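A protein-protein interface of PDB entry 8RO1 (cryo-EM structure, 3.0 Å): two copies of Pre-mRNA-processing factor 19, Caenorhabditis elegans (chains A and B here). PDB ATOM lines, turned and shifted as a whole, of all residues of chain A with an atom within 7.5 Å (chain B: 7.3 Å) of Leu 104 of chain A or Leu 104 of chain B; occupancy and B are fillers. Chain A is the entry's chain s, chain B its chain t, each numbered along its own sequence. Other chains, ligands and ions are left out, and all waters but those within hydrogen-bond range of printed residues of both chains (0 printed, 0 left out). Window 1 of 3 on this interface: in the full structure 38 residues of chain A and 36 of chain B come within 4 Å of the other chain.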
ATOM      1  N   GLN A  98       3.824  21.213  -9.510  1.00  0.00           N
ATOM      2  CA  GLN A  98       2.409  21.337  -9.842  1.00  0.00           C
ATOM      3  C   GLN A  98       1.924  20.161 -10.677  1.00  0.00           C
ATOM      4  O   GLN A  98       0.834  19.630 -10.435  1.00  0.00           O
ATOM      5  CB  GLN A  98       2.154  22.648 -10.581  1.00  0.00           C
ATOM      6  CG  GLN A  98       2.269  23.884  -9.706  1.00  0.00           C
ATOM      7  CD  GLN A  98       2.188  25.172 -10.503  1.00  0.00           C
ATOM      8  OE1 GLN A  98       2.031  25.152 -11.723  1.00  0.00           O
ATOM      9  NE2 GLN A  98       2.304  26.302  -9.815  1.00  0.00           N
ATOM     10  N   ILE A  99       2.711  19.744 -11.666  1.00  0.00           N
ATOM     11  CA  ILE A  99       2.323  18.617 -12.512  1.00  0.00           C
ATOM     12  C   ILE A  99       2.243  17.330 -11.699  1.00  0.00           C
ATOM     13  O   ILE A  99       1.316  16.532 -11.874  1.00  0.00           O
ATOM     14  CB  ILE A  99       3.286  18.490 -13.712  1.00  0.00           C
ATOM     15  CG1 ILE A  99       3.133  19.704 -14.638  1.00  0.00           C
ATOM     16  CG2 ILE A  99       3.019  17.201 -14.520  1.00  0.00           C
ATOM     17  CD1 ILE A  99       4.241  19.868 -15.664  1.00  0.00           C
ATOM     18  N   ALA A 100       3.217  17.092 -10.818  1.00  0.00           N
ATOM     19  CA  ALA A 100       3.204  15.868 -10.019  1.00  0.00           C
ATOM     20  C   ALA A 100       1.998  15.811  -9.094  1.00  0.00           C
ATOM     21  O   ALA A 100       1.356  14.763  -8.966  1.00  0.00           O
ATOM     22  CB  ALA A 100       4.492  15.755  -9.207  1.00  0.00           C
ATOM     23  N   ARG A 101       1.674  16.919  -8.434  1.00  0.00           N
ATOM     24  CA  ARG A 101       0.497  16.944  -7.574  1.00  0.00           C
ATOM     25  C   ARG A 101      -0.792  16.846  -8.369  1.00  0.00           C
ATOM     26  O   ARG A 101      -1.780  16.296  -7.876  1.00  0.00           O
ATOM     27  CB  ARG A 101       0.491  18.206  -6.729  1.00  0.00           C
ATOM     28  CG  ARG A 101       1.505  18.170  -5.620  1.00  0.00           C
ATOM     29  CD  ARG A 101       1.522  19.457  -4.850  1.00  0.00           C
ATOM     30  NE  ARG A 101       0.296  19.612  -4.069  1.00  0.00           N
ATOM     31  CZ  ARG A 101       0.195  19.631  -2.744  1.00  0.00           C
ATOM     32  NH1 ARG A 101      -1.001  19.811  -2.192  1.00  0.00           N
ATOM     33  NH2 ARG A 101       1.248  19.505  -1.953  1.00  0.00           N
ATOM     34  N   GLN A 102      -0.813  17.381  -9.583  1.00  0.00           N
ATOM     35  CA  GLN A 102      -1.974  17.197 -10.443  1.00  0.00           C
ATOM     36  C   GLN A 102      -2.144  15.735 -10.825  1.00  0.00           C
ATOM     37  O   GLN A 102      -3.248  15.189 -10.745  1.00  0.00           O
ATOM     38  CB  GLN A 102      -1.844  18.077 -11.686  1.00  0.00           C
ATOM     39  CG  GLN A 102      -2.990  17.956 -12.679  1.00  0.00           C
ATOM     40  CD  GLN A 102      -2.933  19.011 -13.767  1.00  0.00           C
ATOM     41  OE1 GLN A 102      -2.126  19.937 -13.708  1.00  0.00           O
ATOM     42  NE2 GLN A 102      -3.796  18.879 -14.766  1.00  0.00           N
ATOM     43  N   GLU A 103      -1.067  15.087 -11.265  1.00  0.00           N
ATOM     44  CA  GLU A 103      -1.174  13.686 -11.657  1.00  0.00           C
ATOM     45  C   GLU A 103      -1.450  12.761 -10.477  1.00  0.00           C
ATOM     46  O   GLU A 103      -2.162  11.766 -10.638  1.00  0.00           O
ATOM     47  CB  GLU A 103       0.099  13.251 -12.376  1.00  0.00           C
ATOM     48  CG  GLU A 103       0.258  13.881 -13.746  1.00  0.00           C
ATOM     49  CD  GLU A 103       1.360  13.238 -14.559  1.00  0.00           C
ATOM     50  OE1 GLU A 103       2.330  12.736 -13.956  1.00  0.00           O
ATOM     51  OE2 GLU A 103       1.262  13.242 -15.804  1.00  0.00           O
ATOM     52  N   LEU A 104      -0.909  13.055  -9.296  1.00  0.00           N
ATOM     53  CA  LEU A 104      -1.210  12.233  -8.125  1.00  0.00           C
ATOM     54  C   LEU A 104      -2.681  12.298  -7.737  1.00  0.00           C
ATOM     55  O   LEU A 104      -3.257  11.292  -7.315  1.00  0.00           O
ATOM     56  CB  LEU A 104      -0.338  12.659  -6.947  1.00  0.00           C
ATOM     57  CG  LEU A 104      -0.538  11.982  -5.589  1.00  0.00           C
ATOM     58  CD1 LEU A 104      -0.355  10.492  -5.660  1.00  0.00           C
ATOM     59  CD2 LEU A 104       0.435  12.558  -4.591  1.00  0.00           C
ATOM     60  N   SER A 105      -3.294  13.477  -7.824  1.00  0.00           N
ATOM     61  CA  SER A 105      -4.722  13.587  -7.542  1.00  0.00           C
ATOM     62  C   SER A 105      -5.547  12.749  -8.503  1.00  0.00           C
ATOM     63  O   SER A 105      -6.506  12.087  -8.096  1.00  0.00           O
ATOM     64  CB  SER A 105      -5.169  15.043  -7.597  1.00  0.00           C
ATOM     65  OG  SER A 105      -4.454  15.822  -6.662  1.00  0.00           O
ATOM     66  N   HIS A 106      -5.199  12.775  -9.786  1.00  0.00           N
ATOM     67  CA  HIS A 106      -5.877  11.926 -10.756  1.00  0.00           C
ATOM     68  C   HIS A 106      -5.621  10.452 -10.478  1.00  0.00           C
ATOM     69  O   HIS A 106      -6.538   9.632 -10.577  1.00  0.00           O
ATOM     70  CB  HIS A 106      -5.422  12.291 -12.163  1.00  0.00           C
ATOM     71  CG  HIS A 106      -6.114  11.522 -13.240  1.00  0.00           C
ATOM     72  ND1 HIS A 106      -7.421  11.767 -13.600  1.00  0.00           N
ATOM     73  CD2 HIS A 106      -5.685  10.516 -14.038  1.00  0.00           C
ATOM     74  CE1 HIS A 106      -7.769  10.944 -14.573  1.00  0.00           C
ATOM     75  NE2 HIS A 106      -6.735  10.175 -14.858  1.00  0.00           N
ATOM     76  N   SER A 107      -4.380  10.093 -10.152  1.00  0.00           N
ATOM     77  CA  SER A 107      -4.056   8.697  -9.873  1.00  0.00           C
ATOM     78  C   SER A 107      -4.821   8.165  -8.669  1.00  0.00           C
ATOM     79  O   SER A 107      -5.378   7.065  -8.714  1.00  0.00           O
ATOM     80  CB  SER A 107      -2.559   8.546  -9.637  1.00  0.00           C
ATOM     81  OG  SER A 107      -2.217   7.187  -9.459  1.00  0.00           O
ATOM     82  N   LEU A 108      -4.857   8.929  -7.579  1.00  0.00           N
ATOM     83  CA  LEU A 108      -5.612   8.497  -6.407  1.00  0.00           C
ATOM     84  C   LEU A 108      -7.105   8.443  -6.692  1.00  0.00           C
ATOM     85  O   LEU A 108      -7.813   7.591  -6.149  1.00  0.00           O
ATOM     86  CB  LEU A 108      -5.332   9.428  -5.230  1.00  0.00           C
ATOM     87  CG  LEU A 108      -3.934   9.332  -4.615  1.00  0.00           C
ATOM     88  CD1 LEU A 108      -3.690  10.495  -3.681  1.00  0.00           C
ATOM     89  CD2 LEU A 108      -3.709   8.017  -3.900  1.00  0.00           C
ATOM     90  N   TYR A 109      -7.606   9.364  -7.510  1.00  0.00           N
ATOM     91  CA  TYR A 109      -9.005   9.314  -7.919  1.00  0.00           C
ATOM     92  C   TYR A 109      -9.315   8.032  -8.672  1.00  0.00           C
ATOM     93  O   TYR A 109     -10.324   7.371  -8.406  1.00  0.00           O
ATOM     94  CB  TYR A 109      -9.323  10.535  -8.772  1.00  0.00           C
ATOM     95  CG  TYR A 109     -10.585  10.444  -9.578  1.00  0.00           C
ATOM     96  CD1 TYR A 109     -11.803  10.212  -8.983  1.00  0.00           C
ATOM     97  CD2 TYR A 109     -10.554  10.620 -10.947  1.00  0.00           C
ATOM     98  CE1 TYR A 109     -12.949  10.128  -9.731  1.00  0.00           C
ATOM     99  CE2 TYR A 109     -11.690  10.548 -11.695  1.00  0.00           C
ATOM    100  CZ  TYR A 109     -12.884  10.303 -11.089  1.00  0.00           C
ATOM    101  OH  TYR A 109     -14.013  10.246 -11.864  1.00  0.00           O
ATOM    102  N   GLN A 110      -8.455   7.659  -9.615  1.00  0.00           N
ATOM    103  CA  GLN A 110      -8.684   6.438 -10.371  1.00  0.00           C
ATOM    104  C   GLN A 110      -8.564   5.201  -9.494  1.00  0.00           C
ATOM    105  O   GLN A 110      -9.334   4.249  -9.653  1.00  0.00           O
ATOM    106  CB  GLN A 110      -7.701   6.355 -11.534  1.00  0.00           C
ATOM    107  CG  GLN A 110      -7.930   7.381 -12.615  1.00  0.00           C
ATOM    108  CD  GLN A 110      -9.197   7.124 -13.384  1.00  0.00           C
ATOM    109  OE1 GLN A 110      -9.331   6.102 -14.052  1.00  0.00           O
ATOM    110  NE2 GLN A 110     -10.141   8.044 -13.294  1.00  0.00           N
ATOM    111  N   GLN B  98      10.143  15.187  -4.853  1.00  0.00           N
ATOM    112  CA  GLN B  98      10.493  13.780  -4.683  1.00  0.00           C
ATOM    113  C   GLN B  98       9.453  13.022  -3.867  1.00  0.00           C
ATOM    114  O   GLN B  98       9.164  11.855  -4.153  1.00  0.00           O
ATOM    115  CB  GLN B  98      11.869  13.660  -4.037  1.00  0.00           C
ATOM    116  CG  GLN B  98      13.004  13.931  -5.007  1.00  0.00           C
ATOM    117  CD  GLN B  98      14.368  13.721  -4.386  1.00  0.00           C
ATOM    118  OE1 GLN B  98      14.521  13.766  -3.167  1.00  0.00           O
ATOM    119  NE2 GLN B  98      15.373  13.502  -5.226  1.00  0.00           N
ATOM    120  N   ILE B  99       8.870  13.664  -2.856  1.00  0.00           N
ATOM    121  CA  ILE B  99       7.765  13.048  -2.121  1.00  0.00           C
ATOM    122  C   ILE B  99       6.557  12.846  -3.029  1.00  0.00           C
ATOM    123  O   ILE B  99       5.944  11.775  -3.038  1.00  0.00           O
ATOM    124  CB  ILE B  99       7.423  13.882  -0.870  1.00  0.00           C
ATOM    125  CG1 ILE B  99       8.572  13.786   0.143  1.00  0.00           C
ATOM    126  CG2 ILE B  99       6.100  13.423  -0.209  1.00  0.00           C
ATOM    127  CD1 ILE B  99       8.518  14.796   1.271  1.00  0.00           C
ATOM    128  N   ALA B 100       6.190  13.872  -3.796  1.00  0.00           N
ATOM    129  CA  ALA B 100       5.068  13.739  -4.720  1.00  0.00           C
ATOM    130  C   ALA B 100       5.318  12.662  -5.766  1.00  0.00           C
ATOM    131  O   ALA B 100       4.411  11.896  -6.103  1.00  0.00           O
ATOM    132  CB  ALA B 100       4.792  15.075  -5.404  1.00  0.00           C
ATOM    133  N   ARG B 101       6.532  12.591  -6.299  1.00  0.00           N
ATOM    134  CA  ARG B 101       6.844  11.537  -7.255  1.00  0.00           C
ATOM    135  C   ARG B 101       6.856  10.159  -6.610  1.00  0.00           C
ATOM    136  O   ARG B 101       6.510   9.173  -7.265  1.00  0.00           O
ATOM    137  CB  ARG B 101       8.188  11.822  -7.907  1.00  0.00           C
ATOM    138  CG  ARG B 101       8.128  12.933  -8.924  1.00  0.00           C
ATOM    139  CD  ARG B 101       9.514  13.354  -9.344  1.00  0.00           C
ATOM    140  NE  ARG B 101      10.200  12.296 -10.075  1.00  0.00           N
ATOM    141  CZ  ARG B 101      11.368  12.429 -10.689  1.00  0.00           C
ATOM    142  NH1 ARG B 101      11.884  11.384 -11.327  1.00  0.00           N
ATOM    143  NH2 ARG B 101      12.037  13.573 -10.680  1.00  0.00           N
ATOM    144  N   GLN B 102       7.274  10.060  -5.351  1.00  0.00           N
ATOM    145  CA  GLN B 102       7.170   8.789  -4.640  1.00  0.00           C
ATOM    146  C   GLN B 102       5.716   8.351  -4.489  1.00  0.00           C
ATOM    147  O   GLN B 102       5.369   7.205  -4.794  1.00  0.00           O
ATOM    148  CB  GLN B 102       7.856   8.901  -3.280  1.00  0.00           C
ATOM    149  CG  GLN B 102       7.726   7.677  -2.379  1.00  0.00           C
ATOM    150  CD  GLN B 102       8.196   6.395  -3.043  1.00  0.00           C
ATOM    151  OE1 GLN B 102       7.550   5.357  -2.917  1.00  0.00           O
ATOM    152  NE2 GLN B 102       9.316   6.457  -3.753  1.00  0.00           N
ATOM    153  N   GLU B 103       4.845   9.254  -4.034  1.00  0.00           N
ATOM    154  CA  GLU B 103       3.431   8.922  -3.895  1.00  0.00           C
ATOM    155  C   GLU B 103       2.770   8.661  -5.235  1.00  0.00           C
ATOM    156  O   GLU B 103       1.839   7.855  -5.314  1.00  0.00           O
ATOM    157  CB  GLU B 103       2.683  10.048  -3.183  1.00  0.00           C
ATOM    158  CG  GLU B 103       3.134  10.364  -1.765  1.00  0.00           C
ATOM    159  CD  GLU B 103       3.178   9.155  -0.862  1.00  0.00           C
ATOM    160  OE1 GLU B 103       2.304   8.277  -1.010  1.00  0.00           O
ATOM    161  OE2 GLU B 103       4.081   9.083  -0.002  1.00  0.00           O
ATOM    162  N   LEU B 104       3.225   9.323  -6.291  1.00  0.00           N
ATOM    163  CA  LEU B 104       2.705   9.026  -7.618  1.00  0.00           C
ATOM    164  C   LEU B 104       3.071   7.609  -8.023  1.00  0.00           C
ATOM    165  O   LEU B 104       2.244   6.882  -8.581  1.00  0.00           O
ATOM    166  CB  LEU B 104       3.226  10.045  -8.628  1.00  0.00           C
ATOM    167  CG  LEU B 104       2.876   9.863 -10.103  1.00  0.00           C
ATOM    168  CD1 LEU B 104       1.387   9.936 -10.312  1.00  0.00           C
ATOM    169  CD2 LEU B 104       3.562  10.924 -10.926  1.00  0.00           C
ATOM    170  N   SER B 105       4.320   7.211  -7.781  1.00  0.00           N
ATOM    171  CA  SER B 105       4.745   5.857  -8.116  1.00  0.00           C
ATOM    172  C   SER B 105       3.947   4.806  -7.357  1.00  0.00           C
ATOM    173  O   SER B 105       3.532   3.800  -7.939  1.00  0.00           O
ATOM    174  CB  SER B 105       6.232   5.693  -7.819  1.00  0.00           C
ATOM    175  OG  SER B 105       6.687   4.413  -8.215  1.00  0.00           O
ATOM    176  N   HIS B 106       3.721   5.013  -6.062  1.00  0.00           N
ATOM    177  CA  HIS B 106       2.909   4.061  -5.311  1.00  0.00           C
ATOM    178  C   HIS B 106       1.466   4.041  -5.792  1.00  0.00           C
ATOM    179  O   HIS B 106       0.865   2.971  -5.916  1.00  0.00           O
ATOM    180  CB  HIS B 106       2.959   4.371  -3.821  1.00  0.00           C
ATOM    181  CG  HIS B 106       2.417   3.266  -2.974  1.00  0.00           C
ATOM    182  ND1 HIS B 106       3.015   2.028  -2.897  1.00  0.00           N
ATOM    183  CD2 HIS B 106       1.317   3.203  -2.186  1.00  0.00           C
ATOM    184  CE1 HIS B 106       2.309   1.249  -2.096  1.00  0.00           C
ATOM    185  NE2 HIS B 106       1.276   1.940  -1.647  1.00  0.00           N
ATOM    186  N   SER B 107       0.892   5.210  -6.059  1.00  0.00           N
ATOM    187  CA  SER B 107      -0.491   5.274  -6.519  1.00  0.00           C
ATOM    188  C   SER B 107      -0.682   4.605  -7.871  1.00  0.00           C
ATOM    189  O   SER B 107      -1.727   3.999  -8.120  1.00  0.00           O
ATOM    190  CB  SER B 107      -0.954   6.722  -6.597  1.00  0.00           C
ATOM    191  OG  SER B 107      -2.310   6.780  -7.001  1.00  0.00           O
ATOM    192  N   LEU B 108       0.300   4.715  -8.764  1.00  0.00           N
ATOM    193  CA  LEU B 108       0.177   4.040 -10.052  1.00  0.00           C
ATOM    194  C   LEU B 108       0.223   2.525  -9.922  1.00  0.00           C
ATOM    195  O   LEU B 108      -0.565   1.824 -10.565  1.00  0.00           O
ATOM    196  CB  LEU B 108       1.284   4.513 -10.989  1.00  0.00           C
ATOM    197  CG  LEU B 108       1.182   5.943 -11.517  1.00  0.00           C
ATOM    198  CD1 LEU B 108       2.476   6.351 -12.194  1.00  0.00           C
ATOM    199  CD2 LEU B 108       0.018   6.095 -12.484  1.00  0.00           C
ATOM    200  N   TYR B 109       1.141   1.993  -9.119  1.00  0.00           N
ATOM    201  CA  TYR B 109       1.165   0.551  -8.899  1.00  0.00           C
ATOM    202  C   TYR B 109      -0.020   0.053  -8.082  1.00  0.00           C
ATOM    203  O   TYR B 109      -0.489  -1.068  -8.306  1.00  0.00           O
ATOM    204  CB  TYR B 109       2.489   0.138  -8.252  1.00  0.00           C
ATOM    205  CG  TYR B 109       3.664   0.113  -9.214  1.00  0.00           C
ATOM    206  CD1 TYR B 109       3.645  -0.677 -10.357  1.00  0.00           C
ATOM    207  CD2 TYR B 109       4.784   0.885  -8.987  1.00  0.00           C
ATOM    208  CE1 TYR B 109       4.697  -0.693 -11.228  1.00  0.00           C
ATOM    209  CE2 TYR B 109       5.842   0.872  -9.855  1.00  0.00           C
ATOM    210  CZ  TYR B 109       5.794   0.079 -10.974  1.00  0.00           C
ATOM    211  OH  TYR B 109       6.849   0.058 -11.854  1.00  0.00           O
ATOM    212  N   GLN B 110      -0.539   0.853  -7.154  1.00  0.00           N
ATOM    213  CA  GLN B 110      -1.765   0.455  -6.470  1.00  0.00           C
ATOM    214  C   GLN B 110      -2.956   0.437  -7.414  1.00  0.00           C
ATOM    215  O   GLN B 110      -3.811  -0.445  -7.319  1.00  0.00           O
ATOM    216  CB  GLN B 110      -2.037   1.391  -5.301  1.00  0.00           C
ATOM    217  CG  GLN B 110      -1.104   1.192  -4.133  1.00  0.00           C
ATOM    218  CD  GLN B 110      -1.542   0.069  -3.227  1.00  0.00           C
ATOM    219  OE1 GLN B 110      -1.649  -1.077  -3.654  1.00  0.00           O
ATOM    220  NE2 GLN B 110      -1.795   0.391  -1.965  1.00  0.00           N
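The side-chain hydroxyl (OG) of Ser 107 of chain B sits at hydrogen-bond distance from the side-chain hydroxyl (OG) of Ser 107 of chain A, at 2.5 Å. The side-chain hydroxyl (OG) of Ser 107 of chain B is in hydrogen-bond range of the backbone NH (N) of Leu 108 of chain A.
Ala 100 of chain A touches Ala 100 of chain B (CB to CB, 3.9 Å). Glu 103 of chain A touches Leu 104 of chain B (OE1 to CD2, 3.7 Å). CD1 of Leu 104 of chain A touches O of Glu 103 of chain B, 3.4 Å away. Leu 104 of chain A touches Leu 104 of chain B (CD1 to N, 3.8 Å). CB of Ser 107 of chain B touches CD1 of Leu 104 of chain A, 3.9 Å away. Leu 108 of chain B touches Ser 107 of chain A.
Of the printed residues of chain B, Ala 100 of chain A touches Ala 100. Of chain B, only Glu 103 (3.4 Å), Leu 104 (3.8 Å) and Ser 107 (3.9 Å) come within 4 Å of Leu 104 of chain A. Printed residues of chain B within 4 Å of Leu 108 of chain A: Ser 107. Arg 101 of chain B touches none of the printed residues of chain A. Leu 104 of chain B touches just these residues of chain A: Glu 103 and Leu 104. Ser 105 of chain B touches none of the printed residues of chain A. Printed residues of chain A within 4 Å of Ser 107 of chain B: Leu 104, Ser 107 and Leu 108. Of the printed residues of chain A, Leu 108 of chain B touches Ser 107. The nearest residue of chain A that does not touch Leu 104 of chain B is Ser 107 of chain A (4.2 Å).
Of the 13 printed residues of chain B, 5 touch a printed residue of chain A. Hydrophobic or aromatic side chains of chain B that line the printed part of chain A: Ala 100, Leu 104 and Leu 108. Of the 13 printed residues of chain A, 5 touch a printed residue of chain B.
Ala 100 of chain A touches its own counterpart, Ala 100 of chain B. Glu 103 of chain A touches Leu 104 of chain B, and with the chains exchanged Leu 104 of chain A touches Glu 103 of chain B. Ser 107 of chain B touches its own counterpart, Ser 107 of chain A. Ser 107 of chain A touches Leu 108 of chain B, and with the chains exchanged Leu 108 of chain A touches Ser 107 of chain B. Of the 8 pairs that touch across the chains among the printed residues, 7 have their exchanged pair printed and touching as well.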
